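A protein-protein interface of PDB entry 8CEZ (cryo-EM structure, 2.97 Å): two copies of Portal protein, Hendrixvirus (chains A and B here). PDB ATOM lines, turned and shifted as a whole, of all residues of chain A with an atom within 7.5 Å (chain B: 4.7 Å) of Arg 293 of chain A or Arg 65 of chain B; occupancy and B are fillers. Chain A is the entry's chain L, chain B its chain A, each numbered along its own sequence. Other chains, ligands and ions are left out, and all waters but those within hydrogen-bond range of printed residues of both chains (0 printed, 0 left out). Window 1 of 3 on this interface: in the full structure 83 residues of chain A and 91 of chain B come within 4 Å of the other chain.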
ATOM      1  N   THR A  62      14.672 -21.988  23.317  1.00  0.00           N
ATOM      2  CA  THR A  62      13.576 -22.421  24.174  1.00  0.00           C
ATOM      3  C   THR A  62      13.889 -23.761  24.832  1.00  0.00           C
ATOM      4  O   THR A  62      13.759 -23.909  26.051  1.00  0.00           O
ATOM      5  CB  THR A  62      12.288 -22.509  23.358  1.00  0.00           C
ATOM      6  OG1 THR A  62      12.110 -21.294  22.620  1.00  0.00           O
ATOM      7  CG2 THR A  62      11.088 -22.717  24.272  1.00  0.00           C
ATOM      8  N   CYS A  66      14.454 -24.300  28.846  1.00  0.00           N
ATOM      9  CA  CYS A  66      13.575 -25.171  29.619  1.00  0.00           C
ATOM     10  C   CYS A  66      14.380 -26.251  30.333  1.00  0.00           C
ATOM     11  O   CYS A  66      14.257 -26.441  31.553  1.00  0.00           O
ATOM     12  CB  CYS A  66      12.532 -25.804  28.697  1.00  0.00           C
ATOM     13  SG  CYS A  66      11.410 -24.643  27.881  1.00  0.00           S
ATOM     14  N   PHE A 186       7.017 -40.242  32.161  1.00  0.00           N
ATOM     15  CA  PHE A 186       5.600 -40.545  32.308  1.00  0.00           C
ATOM     16  C   PHE A 186       5.076 -41.479  31.224  1.00  0.00           C
ATOM     17  O   PHE A 186       3.859 -41.637  31.096  1.00  0.00           O
ATOM     18  CB  PHE A 186       4.772 -39.255  32.322  1.00  0.00           C
ATOM     19  CG  PHE A 186       4.565 -38.643  30.965  1.00  0.00           C
ATOM     20  CD1 PHE A 186       5.454 -37.717  30.465  1.00  0.00           C
ATOM     21  CD2 PHE A 186       3.458 -38.980  30.201  1.00  0.00           C
ATOM     22  CE1 PHE A 186       5.254 -37.157  29.227  1.00  0.00           C
ATOM     23  CE2 PHE A 186       3.260 -38.426  28.963  1.00  0.00           C
ATOM     24  CZ  PHE A 186       4.156 -37.511  28.477  1.00  0.00           C
ATOM     25  N   PHE A 286       4.905 -18.013  18.505  1.00  0.00           N
ATOM     26  CA  PHE A 286       4.032 -19.153  18.747  1.00  0.00           C
ATOM     27  C   PHE A 286       4.832 -20.442  18.843  1.00  0.00           C
ATOM     28  O   PHE A 286       4.466 -21.340  19.604  1.00  0.00           O
ATOM     29  CB  PHE A 286       2.979 -19.269  17.648  1.00  0.00           C
ATOM     30  CG  PHE A 286       1.911 -20.282  17.947  1.00  0.00           C
ATOM     31  CD1 PHE A 286       0.939 -20.022  18.895  1.00  0.00           C
ATOM     32  CD2 PHE A 286       1.892 -21.500  17.297  1.00  0.00           C
ATOM     33  CE1 PHE A 286      -0.036 -20.951  19.177  1.00  0.00           C
ATOM     34  CE2 PHE A 286       0.920 -22.431  17.578  1.00  0.00           C
ATOM     35  CZ  PHE A 286      -0.043 -22.157  18.519  1.00  0.00           C
ATOM     36  N   GLN A 287       5.923 -20.550  18.092  1.00  0.00           N
ATOM     37  CA  GLN A 287       6.769 -21.728  18.202  1.00  0.00           C
ATOM     38  C   GLN A 287       7.536 -21.755  19.515  1.00  0.00           C
ATOM     39  O   GLN A 287       7.780 -22.835  20.060  1.00  0.00           O
ATOM     40  CB  GLN A 287       7.735 -21.792  17.021  1.00  0.00           C
ATOM     41  CG  GLN A 287       8.225 -23.193  16.707  1.00  0.00           C
ATOM     42  CD  GLN A 287       7.097 -24.153  16.393  1.00  0.00           C
ATOM     43  OE1 GLN A 287       7.083 -25.281  16.875  1.00  0.00           O
ATOM     44  NE2 GLN A 287       6.149 -23.713  15.578  1.00  0.00           N
ATOM     45  N   VAL A 288       7.926 -20.593  20.038  1.00  0.00           N
ATOM     46  CA  VAL A 288       8.469 -20.554  21.395  1.00  0.00           C
ATOM     47  C   VAL A 288       7.477 -21.174  22.370  1.00  0.00           C
ATOM     48  O   VAL A 288       7.841 -21.994  23.220  1.00  0.00           O
ATOM     49  CB  VAL A 288       8.831 -19.114  21.799  1.00  0.00           C
ATOM     50  CG1 VAL A 288       9.235 -19.065  23.256  1.00  0.00           C
ATOM     51  CG2 VAL A 288       9.965 -18.589  20.943  1.00  0.00           C
ATOM     52  N   SER A 289       6.205 -20.796  22.253  1.00  0.00           N
ATOM     53  CA  SER A 289       5.193 -21.364  23.148  1.00  0.00           C
ATOM     54  C   SER A 289       5.017 -22.867  22.919  1.00  0.00           C
ATOM     55  O   SER A 289       4.913 -23.649  23.876  1.00  0.00           O
ATOM     56  CB  SER A 289       3.864 -20.635  22.963  1.00  0.00           C
ATOM     57  OG  SER A 289       3.237 -21.030  21.757  1.00  0.00           O
ATOM     58  N   GLU A 290       4.994 -23.288  21.651  1.00  0.00           N
ATOM     59  CA  GLU A 290       4.814 -24.701  21.329  1.00  0.00           C
ATOM     60  C   GLU A 290       5.936 -25.551  21.908  1.00  0.00           C
ATOM     61  O   GLU A 290       5.692 -26.646  22.424  1.00  0.00           O
ATOM     62  CB  GLU A 290       4.745 -24.889  19.814  1.00  0.00           C
ATOM     63  CG  GLU A 290       3.445 -24.442  19.184  1.00  0.00           C
ATOM     64  CD  GLU A 290       2.450 -25.576  19.018  1.00  0.00           C
ATOM     65  OE1 GLU A 290       2.865 -26.689  18.641  1.00  0.00           O
ATOM     66  OE2 GLU A 290       1.250 -25.352  19.263  1.00  0.00           O
ATOM     67  N   LEU A 291       7.179 -25.077  21.809  1.00  0.00           N
ATOM     68  CA  LEU A 291       8.302 -25.837  22.341  1.00  0.00           C
ATOM     69  C   LEU A 291       8.376 -25.753  23.859  1.00  0.00           C
ATOM     70  O   LEU A 291       8.852 -26.693  24.503  1.00  0.00           O
ATOM     71  CB  LEU A 291       9.611 -25.347  21.721  1.00  0.00           C
ATOM     72  CG  LEU A 291       9.863 -25.799  20.280  1.00  0.00           C
ATOM     73  CD1 LEU A 291      11.050 -25.067  19.695  1.00  0.00           C
ATOM     74  CD2 LEU A 291      10.081 -27.300  20.205  1.00  0.00           C
ATOM     75  N   ALA A 292       7.924 -24.644  24.448  1.00  0.00           N
ATOM     76  CA  ALA A 292       7.833 -24.576  25.901  1.00  0.00           C
ATOM     77  C   ALA A 292       6.834 -25.587  26.440  1.00  0.00           C
ATOM     78  O   ALA A 292       6.997 -26.081  27.560  1.00  0.00           O
ATOM     79  CB  ALA A 292       7.443 -23.165  26.333  1.00  0.00           C
ATOM     80  N   ARG A 293       5.791 -25.896  25.666  1.00  0.00           N
ATOM     81  CA  ARG A 293       4.791 -26.857  26.131  1.00  0.00           C
ATOM     82  C   ARG A 293       5.401 -28.232  26.396  1.00  0.00           C
ATOM     83  O   ARG A 293       4.996 -28.924  27.336  1.00  0.00           O
ATOM     84  CB  ARG A 293       3.657 -26.978  25.117  1.00  0.00           C
ATOM     85  CG  ARG A 293       2.324 -26.462  25.624  1.00  0.00           C
ATOM     86  CD  ARG A 293       1.213 -26.740  24.636  1.00  0.00           C
ATOM     87  NE  ARG A 293       1.413 -26.048  23.370  1.00  0.00           N
ATOM     88  CZ  ARG A 293       1.187 -24.759  23.173  1.00  0.00           C
ATOM     89  NH1 ARG A 293       0.753 -23.975  24.146  1.00  0.00           N
ATOM     90  NH2 ARG A 293       1.394 -24.241  21.967  1.00  0.00           N
ATOM     91  N   PHE A 294       6.371 -28.650  25.583  1.00  0.00           N
ATOM     92  CA  PHE A 294       6.890 -30.013  25.676  1.00  0.00           C
ATOM     93  C   PHE A 294       7.647 -30.288  26.968  1.00  0.00           C
ATOM     94  O   PHE A 294       7.971 -31.450  27.232  1.00  0.00           O
ATOM     95  CB  PHE A 294       7.797 -30.317  24.486  1.00  0.00           C
ATOM     96  CG  PHE A 294       7.096 -31.001  23.355  1.00  0.00           C
ATOM     97  CD1 PHE A 294       6.849 -32.360  23.403  1.00  0.00           C
ATOM     98  CD2 PHE A 294       6.673 -30.286  22.248  1.00  0.00           C
ATOM     99  CE1 PHE A 294       6.198 -32.990  22.368  1.00  0.00           C
ATOM    100  CE2 PHE A 294       6.025 -30.916  21.212  1.00  0.00           C
ATOM    101  CZ  PHE A 294       5.786 -32.268  21.275  1.00  0.00           C
ATOM    102  N   PHE A 295       7.953 -29.264  27.764  1.00  0.00           N
ATOM    103  CA  PHE A 295       8.666 -29.446  29.018  1.00  0.00           C
ATOM    104  C   PHE A 295       7.908 -28.937  30.235  1.00  0.00           C
ATOM    105  O   PHE A 295       8.324 -29.226  31.362  1.00  0.00           O
ATOM    106  CB  PHE A 295      10.041 -28.766  28.944  1.00  0.00           C
ATOM    107  CG  PHE A 295      10.849 -29.193  27.752  1.00  0.00           C
ATOM    108  CD1 PHE A 295      11.615 -30.346  27.796  1.00  0.00           C
ATOM    109  CD2 PHE A 295      10.819 -28.462  26.580  1.00  0.00           C
ATOM    110  CE1 PHE A 295      12.345 -30.745  26.699  1.00  0.00           C
ATOM    111  CE2 PHE A 295      11.546 -28.859  25.487  1.00  0.00           C
ATOM    112  CZ  PHE A 295      12.308 -30.002  25.545  1.00  0.00           C
ATOM    113  N   GLY A 296       6.812 -28.206  30.050  1.00  0.00           N
ATOM    114  CA  GLY A 296       5.962 -27.819  31.156  1.00  0.00           C
ATOM    115  C   GLY A 296       6.299 -26.502  31.811  1.00  0.00           C
ATOM    116  O   GLY A 296       5.547 -26.058  32.686  1.00  0.00           O
ATOM    117  N   VAL A 297       7.394 -25.863  31.433  1.00  0.00           N
ATOM    118  CA  VAL A 297       7.761 -24.583  32.039  1.00  0.00           C
ATOM    119  C   VAL A 297       6.823 -23.503  31.505  1.00  0.00           C
ATOM    120  O   VAL A 297       6.579 -23.456  30.288  1.00  0.00           O
ATOM    121  CB  VAL A 297       9.220 -24.244  31.743  1.00  0.00           C
ATOM    122  CG1 VAL A 297       9.396 -23.832  30.304  1.00  0.00           C
ATOM    123  CG2 VAL A 297       9.711 -23.140  32.659  1.00  0.00           C
ATOM    124  N   PRO A 298       6.279 -22.634  32.356  1.00  0.00           N
ATOM    125  CA  PRO A 298       5.375 -21.604  31.854  1.00  0.00           C
ATOM    126  C   PRO A 298       6.105 -20.656  30.925  1.00  0.00           C
ATOM    127  O   PRO A 298       7.317 -20.417  31.080  1.00  0.00           O
ATOM    128  CB  PRO A 298       4.894 -20.893  33.127  1.00  0.00           C
ATOM    129  CG  PRO A 298       5.695 -21.400  34.243  1.00  0.00           C
ATOM    130  CD  PRO A 298       6.552 -22.515  33.797  1.00  0.00           C
ATOM    131  N   PRO A 299       5.408 -20.094  29.937  1.00  0.00           N
ATOM    132  CA  PRO A 299       6.092 -19.214  28.978  1.00  0.00           C
ATOM    133  C   PRO A 299       6.735 -17.996  29.615  1.00  0.00           C
ATOM    134  O   PRO A 299       7.768 -17.529  29.122  1.00  0.00           O
ATOM    135  CB  PRO A 299       4.980 -18.813  28.003  1.00  0.00           C
ATOM    136  CG  PRO A 299       3.702 -19.155  28.667  1.00  0.00           C
ATOM    137  CD  PRO A 299       3.968 -20.224  29.661  1.00  0.00           C
ATOM    138  N   GLU A 306       4.877 -13.565  27.402  1.00  0.00           N
ATOM    139  CA  GLU A 306       3.587 -14.037  26.923  1.00  0.00           C
ATOM    140  C   GLU A 306       2.507 -13.932  27.994  1.00  0.00           C
ATOM    141  O   GLU A 306       1.450 -13.339  27.759  1.00  0.00           O
ATOM    142  CB  GLU A 306       3.721 -15.483  26.434  1.00  0.00           C
ATOM    143  CG  GLU A 306       2.479 -15.984  25.765  1.00  0.00           C
ATOM    144  CD  GLU A 306       2.541 -17.453  25.418  1.00  0.00           C
ATOM    145  OE1 GLU A 306       3.541 -18.106  25.768  1.00  0.00           O
ATOM    146  OE2 GLU A 306       1.587 -17.954  24.789  1.00  0.00           O
ATOM    147  N   GLN A 324       4.070 -26.530  41.907  1.00  0.00           N
ATOM    148  CA  GLN A 324       2.916 -27.419  41.922  1.00  0.00           C
ATOM    149  C   GLN A 324       2.588 -27.959  40.538  1.00  0.00           C
ATOM    150  O   GLN A 324       1.879 -28.965  40.429  1.00  0.00           O
ATOM    151  CB  GLN A 324       1.703 -26.691  42.494  1.00  0.00           C
ATOM    152  CG  GLN A 324       1.794 -26.425  43.980  1.00  0.00           C
ATOM    153  CD  GLN A 324       0.743 -25.453  44.458  1.00  0.00           C
ATOM    154  OE1 GLN A 324       0.353 -24.536  43.737  1.00  0.00           O
ATOM    155  NE2 GLN A 324       0.271 -25.651  45.679  1.00  0.00           N
ATOM    156  N   TYR A 325       3.074 -27.316  39.474  1.00  0.00           N
ATOM    157  CA  TYR A 325       2.711 -27.733  38.127  1.00  0.00           C
ATOM    158  C   TYR A 325       3.872 -28.236  37.282  1.00  0.00           C
ATOM    159  O   TYR A 325       3.630 -28.977  36.326  1.00  0.00           O
ATOM    160  CB  TYR A 325       2.022 -26.579  37.388  1.00  0.00           C
ATOM    161  CG  TYR A 325       0.611 -26.348  37.865  1.00  0.00           C
ATOM    162  CD1 TYR A 325      -0.438 -27.105  37.373  1.00  0.00           C
ATOM    163  CD2 TYR A 325       0.329 -25.383  38.820  1.00  0.00           C
ATOM    164  CE1 TYR A 325      -1.726 -26.904  37.810  1.00  0.00           C
ATOM    165  CE2 TYR A 325      -0.953 -25.173  39.259  1.00  0.00           C
ATOM    166  CZ  TYR A 325      -1.977 -25.938  38.755  1.00  0.00           C
ATOM    167  OH  TYR A 325      -3.260 -25.727  39.192  1.00  0.00           O
ATOM    168  N   THR A 326       5.109 -27.867  37.597  1.00  0.00           N
ATOM    169  CA  THR A 326       6.257 -28.295  36.806  1.00  0.00           C
ATOM    170  C   THR A 326       7.261 -29.131  37.581  1.00  0.00           C
ATOM    171  O   THR A 326       7.592 -30.238  37.151  1.00  0.00           O
ATOM    172  CB  THR A 326       6.975 -27.069  36.223  1.00  0.00           C
ATOM    173  OG1 THR A 326       6.020 -26.203  35.598  1.00  0.00           O
ATOM    174  CG2 THR A 326       8.020 -27.491  35.201  1.00  0.00           C
ATOM    175  N   PRO A 329       6.821 -33.237  39.949  1.00  0.00           N
ATOM    176  CA  PRO A 329       7.111 -34.583  39.427  1.00  0.00           C
ATOM    177  C   PRO A 329       8.566 -34.998  39.547  1.00  0.00           C
ATOM    178  O   PRO A 329       8.834 -36.148  39.898  1.00  0.00           O
ATOM    179  CB  PRO A 329       6.667 -34.482  37.965  1.00  0.00           C
ATOM    180  CG  PRO A 329       5.616 -33.454  37.963  1.00  0.00           C
ATOM    181  CD  PRO A 329       5.970 -32.464  39.030  1.00  0.00           C
ATOM    182  N   SER B  61       2.243 -30.608  20.664  1.00  0.00           N
ATOM    183  CA  SER B  61       2.660 -30.097  21.967  1.00  0.00           C
ATOM    184  C   SER B  61       1.481 -29.980  22.921  1.00  0.00           C
ATOM    185  O   SER B  61       1.625 -30.213  24.126  1.00  0.00           O
ATOM    186  CB  SER B  61       3.349 -28.746  21.805  1.00  0.00           C
ATOM    187  OG  SER B  61       2.473 -27.796  21.235  1.00  0.00           O
ATOM    188  N   THR B  62       0.308 -29.625  22.402  1.00  0.00           N
ATOM    189  CA  THR B  62      -0.857 -29.455  23.262  1.00  0.00           C
ATOM    190  C   THR B  62      -1.288 -30.782  23.875  1.00  0.00           C
ATOM    191  O   THR B  62      -1.511 -30.873  25.086  1.00  0.00           O
ATOM    192  CB  THR B  62      -2.002 -28.832  22.465  1.00  0.00           C
ATOM    193  OG1 THR B  62      -1.506 -27.727  21.703  1.00  0.00           O
ATOM    194  CG2 THR B  62      -3.091 -28.335  23.401  1.00  0.00           C
ATOM    195  N   VAL B  63      -1.423 -31.823  23.050  1.00  0.00           N
ATOM    196  CA  VAL B  63      -1.862 -33.123  23.551  1.00  0.00           C
ATOM    197  C   VAL B  63      -0.848 -33.673  24.544  1.00  0.00           C
ATOM    198  O   VAL B  63      -1.203 -34.187  25.614  1.00  0.00           O
ATOM    199  CB  VAL B  63      -2.081 -34.100  22.383  1.00  0.00           C
ATOM    200  CG1 VAL B  63      -2.444 -35.480  22.906  1.00  0.00           C
ATOM    201  CG2 VAL B  63      -3.152 -33.576  21.443  1.00  0.00           C
ATOM    202  N   TRP B  64       0.432 -33.595  24.184  1.00  0.00           N
ATOM    203  CA  TRP B  64       1.492 -34.039  25.076  1.00  0.00           C
ATOM    204  C   TRP B  64       1.395 -33.331  26.417  1.00  0.00           C
ATOM    205  O   TRP B  64       1.446 -33.969  27.474  1.00  0.00           O
ATOM    206  CB  TRP B  64       2.851 -33.787  24.418  1.00  0.00           C
ATOM    207  CG  TRP B  64       4.036 -34.114  25.279  1.00  0.00           C
ATOM    208  CD1 TRP B  64       4.591 -33.325  26.234  1.00  0.00           C
ATOM    209  CD2 TRP B  64       4.816 -35.315  25.251  1.00  0.00           C
ATOM    210  NE1 TRP B  64       5.659 -33.955  26.810  1.00  0.00           N
ATOM    211  CE2 TRP B  64       5.823 -35.179  26.221  1.00  0.00           C
ATOM    212  CE3 TRP B  64       4.761 -36.490  24.499  1.00  0.00           C
ATOM    213  CZ2 TRP B  64       6.765 -36.171  26.463  1.00  0.00           C
ATOM    214  CZ3 TRP B  64       5.696 -37.474  24.742  1.00  0.00           C
ATOM    215  CH2 TRP B  64       6.685 -37.309  25.717  1.00  0.00           C
ATOM    216  N   ARG B  65       1.250 -32.005  26.392  1.00  0.00           N
ATOM    217  CA  ARG B  65       1.191 -31.249  27.636  1.00  0.00           C
ATOM    218  C   ARG B  65      -0.025 -31.636  28.468  1.00  0.00           C
ATOM    219  O   ARG B  65       0.087 -31.827  29.681  1.00  0.00           O
ATOM    220  CB  ARG B  65       1.176 -29.751  27.340  1.00  0.00           C
ATOM    221  CG  ARG B  65       1.136 -28.869  28.577  1.00  0.00           C
ATOM    222  CD  ARG B  65       2.278 -29.167  29.530  1.00  0.00           C
ATOM    223  NE  ARG B  65       2.138 -28.445  30.786  1.00  0.00           N
ATOM    224  CZ  ARG B  65       2.579 -28.880  31.958  1.00  0.00           C
ATOM    225  NH1 ARG B  65       3.200 -30.042  32.078  1.00  0.00           N
ATOM    226  NH2 ARG B  65       2.389 -28.132  33.040  1.00  0.00           N
ATOM    227  N   CYS B  66      -1.195 -31.751  27.842  1.00  0.00           N
ATOM    228  CA  CYS B  66      -2.397 -32.115  28.587  1.00  0.00           C
ATOM    229  C   CYS B  66      -2.221 -33.461  29.277  1.00  0.00           C
ATOM    230  O   CYS B  66      -2.440 -33.594  30.491  1.00  0.00           O
ATOM    231  CB  CYS B  66      -3.599 -32.161  27.643  1.00  0.00           C
ATOM    232  SG  CYS B  66      -4.052 -30.585  26.898  1.00  0.00           S
ATOM    233  N   VAL B  67      -1.822 -34.476  28.509  1.00  0.00           N
ATOM    234  CA  VAL B  67      -1.716 -35.825  29.052  1.00  0.00           C
ATOM    235  C   VAL B  67      -0.656 -35.873  30.147  1.00  0.00           C
ATOM    236  O   VAL B  67      -0.874 -36.443  31.226  1.00  0.00           O
ATOM    237  CB  VAL B  67      -1.418 -36.821  27.918  1.00  0.00           C
ATOM    238  CG1 VAL B  67      -1.182 -38.192  28.466  1.00  0.00           C
ATOM    239  CG2 VAL B  67      -2.569 -36.847  26.929  1.00  0.00           C
ATOM    240  N   SER B  68       0.505 -35.263  29.889  1.00  0.00           N
ATOM    241  CA  SER B  68       1.580 -35.255  30.873  1.00  0.00           C
ATOM    242  C   SER B  68       1.147 -34.555  32.151  1.00  0.00           C
ATOM    243  O   SER B  68       1.388 -35.051  33.256  1.00  0.00           O
ATOM    244  CB  SER B  68       2.812 -34.570  30.279  1.00  0.00           C
ATOM    245  OG  SER B  68       3.791 -34.334  31.271  1.00  0.00           O
ATOM    246  N   LEU B  69       0.508 -33.393  32.022  1.00  0.00           N
ATOM    247  CA  LEU B  69       0.073 -32.654  33.198  1.00  0.00           C
ATOM    248  C   LEU B  69      -0.865 -33.498  34.044  1.00  0.00           C
ATOM    249  O   LEU B  69      -0.649 -33.669  35.249  1.00  0.00           O
ATOM    250  CB  LEU B  69      -0.607 -31.353  32.768  1.00  0.00           C
ATOM    251  CG  LEU B  69      -1.116 -30.429  33.877  1.00  0.00           C
ATOM    252  CD1 LEU B  69       0.030 -29.805  34.658  1.00  0.00           C
ATOM    253  CD2 LEU B  69      -2.011 -29.355  33.300  1.00  0.00           C
ATOM    254  N   VAL B 288      -5.053 -24.961  19.265  1.00  0.00           N
ATOM    255  CA  VAL B 288      -4.566 -25.217  20.617  1.00  0.00           C
ATOM    256  C   VAL B 288      -5.741 -25.279  21.582  1.00  0.00           C
ATOM    257  O   VAL B 288      -5.855 -26.202  22.397  1.00  0.00           O
ATOM    258  CB  VAL B 288      -3.550 -24.138  21.036  1.00  0.00           C
ATOM    259  CG1 VAL B 288      -3.337 -24.157  22.538  1.00  0.00           C
ATOM    260  CG2 VAL B 288      -2.234 -24.339  20.315  1.00  0.00           C
ATOM    261  N   LEU B 301      -3.415 -23.123  31.589  1.00  0.00           N
ATOM    262  CA  LEU B 301      -2.491 -24.072  32.193  1.00  0.00           C
ATOM    263  C   LEU B 301      -1.609 -24.778  31.175  1.00  0.00           C
ATOM    264  O   LEU B 301      -0.585 -25.350  31.559  1.00  0.00           O
ATOM    265  CB  LEU B 301      -3.261 -25.126  32.997  1.00  0.00           C
ATOM    266  CG  LEU B 301      -3.450 -24.856  34.491  1.00  0.00           C
ATOM    267  CD1 LEU B 301      -4.128 -26.039  35.149  1.00  0.00           C
ATOM    268  CD2 LEU B 301      -2.126 -24.558  35.164  1.00  0.00           C
ATOM    269  N   VAL B 302      -1.978 -24.760  29.897  1.00  0.00           N
ATOM    270  CA  VAL B 302      -1.193 -25.388  28.844  1.00  0.00           C
ATOM    271  C   VAL B 302      -0.334 -24.369  28.107  1.00  0.00           C
ATOM    272  O   VAL B 302       0.153 -24.652  27.010  1.00  0.00           O
ATOM    273  CB  VAL B 302      -2.098 -26.165  27.870  1.00  0.00           C
ATOM    274  CG1 VAL B 302      -2.825 -25.221  26.929  1.00  0.00           C
ATOM    275  CG2 VAL B 302      -1.301 -27.199  27.094  1.00  0.00           C
ATOM    276  N   GLY B 303      -0.132 -23.189  28.688  1.00  0.00           N
ATOM    277  CA  GLY B 303       0.709 -22.181  28.077  1.00  0.00           C
ATOM    278  C   GLY B 303       0.089 -21.469  26.899  1.00  0.00           C
ATOM    279  O   GLY B 303       0.810 -21.056  25.986  1.00  0.00           O
ATOM    280  N   ASP B 304      -1.229 -21.299  26.895  1.00  0.00           N
ATOM    281  CA  ASP B 304      -1.943 -20.792  25.733  1.00  0.00           C
ATOM    282  C   ASP B 304      -2.168 -19.284  25.765  1.00  0.00           C
ATOM    283  O   ASP B 304      -2.789 -18.753  24.840  1.00  0.00           O
ATOM    284  CB  ASP B 304      -3.293 -21.505  25.604  1.00  0.00           C
ATOM    285  CG  ASP B 304      -3.981 -21.220  24.285  1.00  0.00           C
ATOM    286  OD1 ASP B 304      -3.296 -20.808  23.327  1.00  0.00           O
ATOM    287  OD2 ASP B 304      -5.211 -21.412  24.205  1.00  0.00           O
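The backbone carbonyl oxygen (O) of Val 302 of chain B sits at hydrogen-bond distance from the guanidinium group (NH1) of Arg 293 of chain A, at 3.0 Å. OE2 of Glu 306 of chain A sits close to O of Gly 303 of chain B. NE1 of Trp 64 of chain B is in hydrogen-bond range of O of Phe 294 of chain A, at 3.4 Å. The guanidinium group (NE) of Arg 293 of chain A is in hydrogen-bond range of the side-chain hydroxyl (OG) of Ser 61 of chain B, 3.0 Å away. OE1 of Glu 290 of chain A lies within hydrogen-bond range of OG of Ser 61 of chain B (2.8 Å). O of Gly 303 of chain B lies within hydrogen-bond range of NH1 of Arg 293 of chain A.
Printed residues of chain B that touch a printed residue of chain A: Ser 61, Thr 62, Trp 64, Arg 65, Ser 68, Leu 69, Val 288, Leu 301, Val 302 and Gly 303. Hydrophobic or aromatic side chains of chain B within 4 Å of the printed part of chain A: Trp 64, Leu 69, Val 288, Leu 301 and Val 302. Among the printed residues, no Asp or Glu carboxylate lies within 4 Å of a Lys or Arg side-chain nitrogen of the other chain.
Phe 186 of chain A touches Trp 64 of chain B (CE1 to CZ2, 3.3 Å). Phe 286 of chain A touches Val 288 of chain B (CZ to CG2, 3.6 Å). Val 288 of chain B touches Glu 290 of chain A. CD of Arg 293 of chain A touches CA of Thr 62 of chain B (3.7 Å). CD of Arg 65 of chain B touches O of Arg 293 of chain A, at 3.5 Å. Arg 293 of chain A touches Val 288 of chain B. CE2 of Phe 294 of chain A touches CB of Ser 61 of chain B (3.5 Å). Gly 296 of chain A touches Arg 65 of chain B. Tyr 325 of chain A touches Arg 65 of chain B. Tyr 325 of chain A touches Leu 301 of chain B.
Of the printed residues of chain B, Phe 294 of chain A touches Ser 61 and Trp 64. Of the printed residues of chain B, Gly 296 of chain A touches Arg 65. Of the printed residues of chain B, Tyr 325 of chain A touches Arg 65 (3.6 Å), Leu 69 (3.9 Å) and Leu 301 (3.6 Å). Arg 65 of chain B touches just these residues of chain A: Arg 293, Gly 296 and Tyr 325. Of the printed residues of chain A, Val 302 of chain B touches Arg 293. The nearest residue of chain A that does not touch Arg 65 of chain B is Thr 326 of chain A (4.8 Å).
The backbone carbonyl oxygen (O) of Thr 62 of chain B lies within hydrogen-bond range of the side-chain sulfur (SG) of Cys 66 of chain B. OG1 of Thr 326 of chain A lies within hydrogen-bond range of O of Gly 296 of chain A, at 3.0 Å. OE2 of Glu 290 of chain A is in salt-bridge range of NH2 of Arg 293 of chain A (2.9 Å). O of Phe 286 of chain A sits at hydrogen-bond distance from OG of Ser 289 of chain A, 2.5 Å away.
3 positions are printed for both chains. Of the 18 pairs that touch across the chains among the printed residues, none has its exchanged pair printed and touching as well.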
